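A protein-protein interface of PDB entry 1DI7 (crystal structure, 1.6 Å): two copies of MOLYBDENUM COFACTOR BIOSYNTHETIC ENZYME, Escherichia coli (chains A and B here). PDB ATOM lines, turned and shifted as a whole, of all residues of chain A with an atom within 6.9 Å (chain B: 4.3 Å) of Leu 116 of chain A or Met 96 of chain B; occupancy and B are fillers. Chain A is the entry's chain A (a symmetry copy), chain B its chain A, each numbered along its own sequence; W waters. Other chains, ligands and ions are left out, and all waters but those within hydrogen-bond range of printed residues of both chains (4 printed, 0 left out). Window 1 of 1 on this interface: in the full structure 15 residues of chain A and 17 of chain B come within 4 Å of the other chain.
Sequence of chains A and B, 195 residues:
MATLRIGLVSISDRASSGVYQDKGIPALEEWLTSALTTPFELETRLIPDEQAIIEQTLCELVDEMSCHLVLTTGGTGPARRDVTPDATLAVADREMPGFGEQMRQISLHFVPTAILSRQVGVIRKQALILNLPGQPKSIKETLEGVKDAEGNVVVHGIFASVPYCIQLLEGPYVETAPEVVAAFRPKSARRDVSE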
ATOM      1  N   THR A  76      36.489  30.447  22.286  1.00  0.00           N
ATOM      2  CA  THR A  76      35.625  31.005  23.340  1.00  0.00           C
ATOM      3  C   THR A  76      34.440  30.134  23.793  1.00  0.00           C
ATOM      4  O   THR A  76      33.625  30.606  24.596  1.00  0.00           O
ATOM      5  CB  THR A  76      35.043  32.363  22.918  1.00  0.00           C
ATOM      6  OG1 THR A  76      34.141  32.192  21.801  1.00  0.00           O
ATOM      7  CG2 THR A  76      36.156  33.337  22.544  1.00  0.00           C
ATOM      8  N   GLY A  77      34.328  28.920  23.290  1.00  0.00           N
ATOM      9  CA  GLY A  77      33.253  28.016  23.685  1.00  0.00           C
ATOM     10  C   GLY A  77      33.412  27.274  24.989  1.00  0.00           C
ATOM     11  O   GLY A  77      34.388  27.501  25.744  1.00  0.00           O
ATOM     12  N   PRO A  78      32.494  26.374  25.319  1.00  0.00           N
ATOM     13  CA  PRO A  78      32.516  25.624  26.581  1.00  0.00           C
ATOM     14  C   PRO A  78      33.497  24.459  26.634  1.00  0.00           C
ATOM     15  O   PRO A  78      33.873  24.022  27.730  1.00  0.00           O
ATOM     16  CB  PRO A  78      31.058  25.112  26.739  1.00  0.00           C
ATOM     17  CG  PRO A  78      30.593  24.974  25.318  1.00  0.00           C
ATOM     18  CD  PRO A  78      31.290  26.081  24.521  1.00  0.00           C
ATOM     19  N   ALA A  79      33.899  23.935  25.480  1.00  0.00           N
ATOM     20  CA  ALA A  79      34.818  22.806  25.438  1.00  0.00           C
ATOM     21  C   ALA A  79      36.078  23.116  26.216  1.00  0.00           C
ATOM     22  O   ALA A  79      36.603  24.226  26.182  1.00  0.00           O
ATOM     23  CB  ALA A  79      35.146  22.445  23.984  1.00  0.00           C
ATOM     24  N   ARG A 104      27.094  38.890  23.800  1.00  0.00           N
ATOM     25  CA  ARG A 104      26.183  37.747  23.781  1.00  0.00           C
ATOM     26  C   ARG A 104      24.772  38.177  23.378  1.00  0.00           C
ATOM     27  O   ARG A 104      24.130  37.484  22.586  1.00  0.00           O
ATOM     28  CB  ARG A 104      26.190  37.000  25.118  1.00  0.00           C
ATOM     29  CG  ARG A 104      27.422  36.138  25.319  1.00  0.00           C
ATOM     30  CD  ARG A 104      27.367  35.344  26.648  1.00  0.00           C
ATOM     31  NE  ARG A 104      27.772  36.140  27.801  1.00  0.00           N
ATOM     32  CZ  ARG A 104      29.007  36.442  28.143  1.00  0.00           C
ATOM     33  NH1 ARG A 104      30.068  35.963  27.458  1.00  0.00           N
ATOM     34  NH2 ARG A 104      29.256  37.207  29.193  1.00  0.00           N
ATOM     35  N   THR A 113      22.969  29.354  19.536  1.00  0.00           N
ATOM     36  CA  THR A 113      23.592  28.992  20.808  1.00  0.00           C
ATOM     37  C   THR A 113      24.588  30.010  21.339  1.00  0.00           C
ATOM     38  O   THR A 113      25.569  29.679  22.025  1.00  0.00           O
ATOM     39  CB  THR A 113      24.296  27.623  20.676  1.00  0.00           C
ATOM     40  OG1 THR A 113      25.247  27.646  19.587  1.00  0.00           O
ATOM     41  CG2 THR A 113      23.279  26.521  20.392  1.00  0.00           C
ATOM     42  N   ALA A 114      24.356  31.301  21.086  1.00  0.00           N
ATOM     43  CA  ALA A 114      25.247  32.360  21.524  1.00  0.00           C
ATOM     44  C   ALA A 114      25.596  32.383  23.008  1.00  0.00           C
ATOM     45  O   ALA A 114      26.731  32.774  23.356  1.00  0.00           O
ATOM     46  CB  ALA A 114      24.640  33.733  21.174  1.00  0.00           C
ATOM     47  N   ILE A 115      24.684  31.984  23.876  1.00  0.00           N
ATOM     48  CA  ILE A 115      24.905  31.970  25.312  1.00  0.00           C
ATOM     49  C   ILE A 115      25.947  30.949  25.772  1.00  0.00           C
ATOM     50  O   ILE A 115      26.331  30.953  26.970  1.00  0.00           O
ATOM     51  CB  ILE A 115      23.607  31.769  26.127  1.00  0.00           C
ATOM     52  CG1 ILE A 115      23.141  30.326  26.057  1.00  0.00           C
ATOM     53  CG2 ILE A 115      22.517  32.751  25.684  1.00  0.00           C
ATOM     54  CD1 ILE A 115      21.951  29.997  26.911  1.00  0.00           C
ATOM     55  N   LEU A 116      26.442  30.116  24.902  1.00  0.00           N
ATOM     56  CA  LEU A 116      27.460  29.133  25.247  1.00  0.00           C
ATOM     57  C   LEU A 116      28.842  29.765  25.191  1.00  0.00           C
ATOM     58  O   LEU A 116      29.851  29.173  25.613  1.00  0.00           O
ATOM     59  CB  LEU A 116      27.403  27.911  24.304  1.00  0.00           C
ATOM     60  CG  LEU A 116      26.119  27.080  24.372  1.00  0.00           C
ATOM     61  CD1 LEU A 116      26.249  25.847  23.488  1.00  0.00           C
ATOM     62  CD2 LEU A 116      25.834  26.638  25.808  1.00  0.00           C
ATOM     63  N   SER A 117      28.926  30.957  24.598  1.00  0.00           N
ATOM     64  CA  SER A 117      30.232  31.642  24.532  1.00  0.00           C
ATOM     65  C   SER A 117      30.620  32.264  25.851  1.00  0.00           C
ATOM     66  O   SER A 117      29.793  32.764  26.632  1.00  0.00           O
ATOM     67  CB  SER A 117      30.133  32.692  23.418  1.00  0.00           C
ATOM     68  OG  SER A 117      30.160  32.005  22.160  1.00  0.00           O
ATOM     69  N   ARG A 118      31.929  32.287  26.134  1.00  0.00           N
ATOM     70  CA  ARG A 118      32.457  32.828  27.354  1.00  0.00           C
ATOM     71  C   ARG A 118      33.337  34.065  27.111  1.00  0.00           C
ATOM     72  O   ARG A 118      34.158  34.431  27.935  1.00  0.00           O
ATOM     73  CB  ARG A 118      33.311  31.730  28.054  1.00  0.00           C
ATOM     74  CG  ARG A 118      32.534  30.428  28.270  1.00  0.00           C
ATOM     75  CD  ARG A 118      33.407  29.294  28.826  1.00  0.00           C
ATOM     76  NE  ARG A 118      33.962  29.601  30.123  1.00  0.00           N
ATOM     77  CZ  ARG A 118      35.223  29.988  30.365  1.00  0.00           C
ATOM     78  NH1 ARG A 118      36.111  30.054  29.396  1.00  0.00           N
ATOM     79  NH2 ARG A 118      35.632  30.273  31.612  1.00  0.00           N
ATOM     80  N   GLN A 119      33.128  34.700  25.961  1.00  0.00           N
ATOM     81  CA  GLN A 119      33.897  35.877  25.577  1.00  0.00           C
ATOM     82  C   GLN A 119      33.888  36.995  26.615  1.00  0.00           C
ATOM     83  O   GLN A 119      32.910  37.197  27.344  1.00  0.00           O
ATOM     84  CB  GLN A 119      33.344  36.401  24.229  1.00  0.00           C
ATOM     85  CG  GLN A 119      32.007  37.120  24.269  1.00  0.00           C
ATOM     86  CD  GLN A 119      30.827  36.252  23.885  1.00  0.00           C
ATOM     87  OE1 GLN A 119      30.121  36.486  22.876  1.00  0.00           O
ATOM     88  NE2 GLN A 119      30.528  35.240  24.667  1.00  0.00           N
ATOM     89  N   ARG B  94      34.682  25.638  35.814  1.00  0.00           N
ATOM     90  CA  ARG B  94      34.628  26.736  34.838  1.00  0.00           C
ATOM     91  C   ARG B  94      33.239  27.375  34.897  1.00  0.00           C
ATOM     92  O   ARG B  94      32.237  26.662  35.056  1.00  0.00           O
ATOM     93  CB  ARG B  94      34.924  26.182  33.427  1.00  0.00           C
ATOM     94  CG  ARG B  94      34.203  26.859  32.264  1.00  0.00           C
ATOM     95  CD  ARG B  94      34.701  26.352  30.916  1.00  0.00           C
ATOM     96  NE  ARG B  94      36.133  26.655  30.691  1.00  0.00           N
ATOM     97  CZ  ARG B  94      36.741  26.469  29.536  1.00  0.00           C
ATOM     98  NH1 ARG B  94      36.052  26.001  28.478  1.00  0.00           N
ATOM     99  NH2 ARG B  94      38.042  26.774  29.397  1.00  0.00           N
ATOM    100  N   GLU B  95      33.187  28.689  34.768  1.00  0.00           N
ATOM    101  CA  GLU B  95      31.937  29.437  34.729  1.00  0.00           C
ATOM    102  C   GLU B  95      31.422  29.668  33.298  1.00  0.00           C
ATOM    103  O   GLU B  95      32.223  29.830  32.375  1.00  0.00           O
ATOM    104  CB  GLU B  95      32.099  30.807  35.396  1.00  0.00           C
ATOM    105  CG  GLU B  95      32.827  30.802  36.726  1.00  0.00           C
ATOM    106  CD  GLU B  95      32.987  32.194  37.305  1.00  0.00           C
ATOM    107  OE1 GLU B  95      32.189  33.099  36.945  1.00  0.00           O
ATOM    108  OE2 GLU B  95      33.919  32.429  38.083  1.00  0.00           O
ATOM    109  N   MET B  96      30.118  29.651  33.129  1.00  0.00           N
ATOM    110  CA  MET B  96      29.420  29.904  31.853  1.00  0.00           C
ATOM    111  C   MET B  96      28.547  31.130  32.076  1.00  0.00           C
ATOM    112  O   MET B  96      27.347  31.016  32.395  1.00  0.00           O
ATOM    113  CB  MET B  96      28.553  28.675  31.490  1.00  0.00           C
ATOM    114  CG  MET B  96      29.369  27.424  31.192  1.00  0.00           C
ATOM    115  SD  MET B  96      30.281  27.583  29.627  1.00  0.00           S
ATOM    116  CE  MET B  96      28.920  27.586  28.482  1.00  0.00           C
ATOM    117  N   PRO B  97      29.099  32.342  31.952  1.00  0.00           N
ATOM    118  CA  PRO B  97      28.385  33.578  32.215  1.00  0.00           C
ATOM    119  C   PRO B  97      27.077  33.766  31.475  1.00  0.00           C
ATOM    120  O   PRO B  97      26.104  34.327  32.021  1.00  0.00           O
ATOM    121  CB  PRO B  97      29.417  34.698  31.914  1.00  0.00           C
ATOM    122  CG  PRO B  97      30.401  34.007  30.961  1.00  0.00           C
ATOM    123  CD  PRO B  97      30.483  32.570  31.487  1.00  0.00           C
ATOM    124  N   GLY B  98      27.044  33.291  30.220  1.00  0.00           N
ATOM    125  CA  GLY B  98      25.817  33.454  29.424  1.00  0.00           C
ATOM    126  C   GLY B  98      24.606  32.771  29.999  1.00  0.00           C
ATOM    127  O   GLY B  98      23.472  33.231  29.796  1.00  0.00           O
ATOM    128  N   PHE B  99      24.781  31.650  30.729  1.00  0.00           N
ATOM    129  CA  PHE B  99      23.590  31.004  31.308  1.00  0.00           C
ATOM    130  C   PHE B  99      22.902  31.830  32.371  1.00  0.00           C
ATOM    131  O   PHE B  99      21.665  31.998  32.347  1.00  0.00           O
ATOM    132  CB  PHE B  99      23.965  29.614  31.870  1.00  0.00           C
ATOM    133  CG  PHE B  99      23.933  28.518  30.834  1.00  0.00           C
ATOM    134  CD1 PHE B  99      25.093  27.856  30.470  1.00  0.00           C
ATOM    135  CD2 PHE B  99      22.740  28.121  30.267  1.00  0.00           C
ATOM    136  CE1 PHE B  99      25.041  26.833  29.541  1.00  0.00           C
ATOM    137  CE2 PHE B  99      22.686  27.099  29.332  1.00  0.00           C
ATOM    138  CZ  PHE B  99      23.845  26.462  28.963  1.00  0.00           C
ATOM    139  N   GLY B 100      23.639  32.403  33.324  1.00  0.00           N
ATOM    140  CA  GLY B 100      23.012  33.226  34.361  1.00  0.00           C
ATOM    141  C   GLY B 100      22.393  34.485  33.718  1.00  0.00           C
ATOM    142  O   GLY B 100      21.258  34.855  34.070  1.00  0.00           O
ATOM    143  N   GLY B 121      25.249  29.184  35.809  1.00  0.00           N
ATOM    144  CA  GLY B 121      25.431  27.924  35.052  1.00  0.00           C
ATOM    145  C   GLY B 121      26.945  27.708  35.081  1.00  0.00           C
ATOM    146  O   GLY B 121      27.714  28.656  34.902  1.00  0.00           O
ATOM    147  N   ILE B 123      30.421  24.505  34.796  1.00  0.00           N
ATOM    148  CA  ILE B 123      30.840  23.161  34.378  1.00  0.00           C
ATOM    149  C   ILE B 123      31.762  22.569  35.484  1.00  0.00           C
ATOM    150  O   ILE B 123      32.634  23.271  35.988  1.00  0.00           O
ATOM    151  CB  ILE B 123      31.634  23.224  33.055  1.00  0.00           C
ATOM    152  CG1 ILE B 123      30.671  23.590  31.900  1.00  0.00           C
ATOM    153  CG2 ILE B 123      32.307  21.889  32.718  1.00  0.00           C
ATOM    154  CD1 ILE B 123      31.437  24.193  30.723  1.00  0.00           C
ATOM    155  N   SER B 161      19.823  25.506  24.102  1.00  0.00           N
ATOM    156  CA  SER B 161      21.267  25.419  23.894  1.00  0.00           C
ATOM    157  C   SER B 161      21.926  24.300  24.699  1.00  0.00           C
ATOM    158  O   SER B 161      23.127  24.069  24.546  1.00  0.00           O
ATOM    159  CB  SER B 161      21.910  26.760  24.297  1.00  0.00           C
ATOM    160  OG  SER B 161      21.315  27.870  23.598  1.00  0.00           O
ATOM    161  N   TYR B 164      23.413  20.885  22.536  1.00  0.00           N
ATOM    162  CA  TYR B 164      24.702  21.170  21.928  1.00  0.00           C
ATOM    163  C   TYR B 164      25.820  21.335  22.947  1.00  0.00           C
ATOM    164  O   TYR B 164      26.940  20.865  22.737  1.00  0.00           O
ATOM    165  CB  TYR B 164      24.622  22.436  21.032  1.00  0.00           C
ATOM    166  CG  TYR B 164      25.836  22.683  20.183  1.00  0.00           C
ATOM    167  CD1 TYR B 164      26.462  21.632  19.495  1.00  0.00           C
ATOM    168  CD2 TYR B 164      26.369  23.946  20.044  1.00  0.00           C
ATOM    169  CE1 TYR B 164      27.583  21.859  18.710  1.00  0.00           C
ATOM    170  CE2 TYR B 164      27.507  24.175  19.271  1.00  0.00           C
ATOM    171  CZ  TYR B 164      28.092  23.132  18.609  1.00  0.00           C
ATOM    172  OH  TYR B 164      29.225  23.382  17.824  1.00  0.00           O
ATOM    173  N   CYS B 165      25.518  21.981  24.094  1.00  0.00           N
ATOM    174  CA  CYS B 165      26.559  22.130  25.122  1.00  0.00           C
ATOM    175  C   CYS B 165      27.022  20.769  25.618  1.00  0.00           C
ATOM    176  O   CYS B 165      28.248  20.528  25.763  1.00  0.00           O
ATOM    177  CB  CYS B 165      26.001  22.953  26.301  1.00  0.00           C
ATOM    178  SG  CYS B 165      27.306  23.524  27.422  1.00  0.00           S
HETATM  179  O   HOH W   1      35.692  29.879  34.639  1.00  0.00           O
HETATM  180  O   HOH W   2      28.451  31.412  28.636  1.00  0.00           O
HETATM  181  O   HOH W   3      21.813  30.860  22.971  1.00  0.00           O
HETATM  182  O   HOH W   4      37.433  28.198  32.798  1.00  0.00           O
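NH1 of Arg 94 of chain B sits at hydrogen-bond distance from O of Pro 78 of chain A, at 3.0 Å.
The backbone carbonyl oxygen (O) of Ala 79 of chain A lies within hydrogen-bond range of the guanidinium group (NH1) of Arg 94 of chain B.
The guanidinium group (NE) of Arg 118 of chain A lies within hydrogen-bond range of the backbone carbonyl oxygen (O) of Glu 95 of chain B (2.9 Å).
N of Ile 123 of chain B lies within hydrogen-bond range of O of Arg 94 of chain B (2.8 Å).
N of Met 96 of chain B sits at hydrogen-bond distance from O of Gly 121 of chain B, 3.1 Å away.
O of Thr 76 of chain A is in hydrogen-bond range of N of Arg 118 of chain A (2.8 Å).
NH1 of Arg 104 of chain A sits at hydrogen-bond distance from O of Ser 117 of chain A (3.3 Å).
The guanidinium group (NH1) of Arg 104 of chain A lies close to the side-chain amide nitrogen (NE2) of Gln 119 of chain A, 2.9 Å away.
Among the printed residues, merely in contact across the chains: Leu 116 of chain A with Met 96 of chain B, Arg 118 of chain A with Arg 94 of chain B, Gly 77 of chain A with Arg 94 of chain B, Ile 115 of chain A with Gly 98 of chain B, Arg 118 of chain A with Met 96 of chain B, Arg 104 of chain A with Gly 98 of chain B, Arg 104 of chain A with Pro 97 of chain B, Pro 78 of chain A with Met 96 of chain B, Leu 116 of chain A with Cys 165 of chain B, Leu 116 of chain A with Phe 99 of chain B, Leu 116 of chain A with Ser 161 of chain B, Thr 113 of chain A with Ser 161 of chain B, Ile 115 of chain A with Phe 99 of chain B, Pro 78 of chain A with Ile 123 of chain B, Thr 113 of chain A with Tyr 164 of chain B, Ile 115 of chain A with Ser 161 of chain B and Leu 116 of chain A with Tyr 164 of chain B.
Leu 116 of chain A touches just these residues of chain B: Met 96, Phe 99, Ser 161, Tyr 164 and Cys 165.
Of chain A, only Pro 78 (3.7 Å), Leu 116 (3.4 Å) and Arg 118 (3.7 Å) come within 4 Å of Met 96 of chain B.
Printed residues of chain A within 4 Å of Glu 95 of chain B: Arg 118 (2.9 Å).
Of the printed residues of chain A, Arg 94 of chain B touches Gly 77, Pro 78, Ala 79 and Arg 118.
Of the printed residues of chain B, Pro 78 of chain A touches Arg 94, Met 96 and Ile 123.
Gly 100 of chain B touches none of the printed residues of chain A.
Ser 117 of chain A touches none of the printed residues of chain B.
The nearest printed residue of chain B that does not touch Leu 116 of chain A is Gly 98 of chain B (5.7 Å).
The nearest residue of chain A that does not touch Met 96 of chain B is Ile 115 of chain A (4.5 Å).
The nearest printed residue of chain A that does not touch Arg 94 of chain B is Thr 76 of chain A (6.5 Å).
Printed residues of chain B that touch a printed residue of chain A: Arg 94, Glu 95, Met 96, Pro 97, Gly 98, Phe 99, Ile 123, Ser 161, Tyr 164 and Cys 165.
Hydrophobic or aromatic side chains of chain B within 4 Å of the printed part of chain A: Met 96, Pro 97, Phe 99, Ile 123 and Tyr 164.
Hydrophobic or aromatic side chains of chain A that line the printed part of chain B: Pro 78, Ile 115 and Leu 116.
Among the printed residues, no Asp or Glu carboxylate lies within 4 Å of a Lys or Arg side-chain nitrogen of the other chain.
No position is printed for both chains.
Of the 20 pairs that touch across the chains among the printed residues, none has its exchanged pair printed and touching as well.
Water W2 lies within hydrogen-bond range of O of Ile 115 of chain A (2.7 Å), O of Ser 117 of chain A (2.8 Å) and N of Gly 98 of chain B (2.8 Å).
Water W1 lies within hydrogen-bond range of the backbone NH of Glu 95 of chain B (2.8 Å) and the guanidinium group of Arg 118 of chain A (3.1 Å).
Water W4 bridges NE of Arg 94 of chain B (2.9 Å) and NH2 of Arg 118 of chain A (3.0 Å).
Water W3 lies within hydrogen-bond range of the side-chain hydroxyl (OG) of Ser 161 of chain B (3.1 Å), the backbone NH (N) of Ala 114 of chain A (3.2 Å) and the backbone NH (N) of Ile 115 of chain A (3.2 Å).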
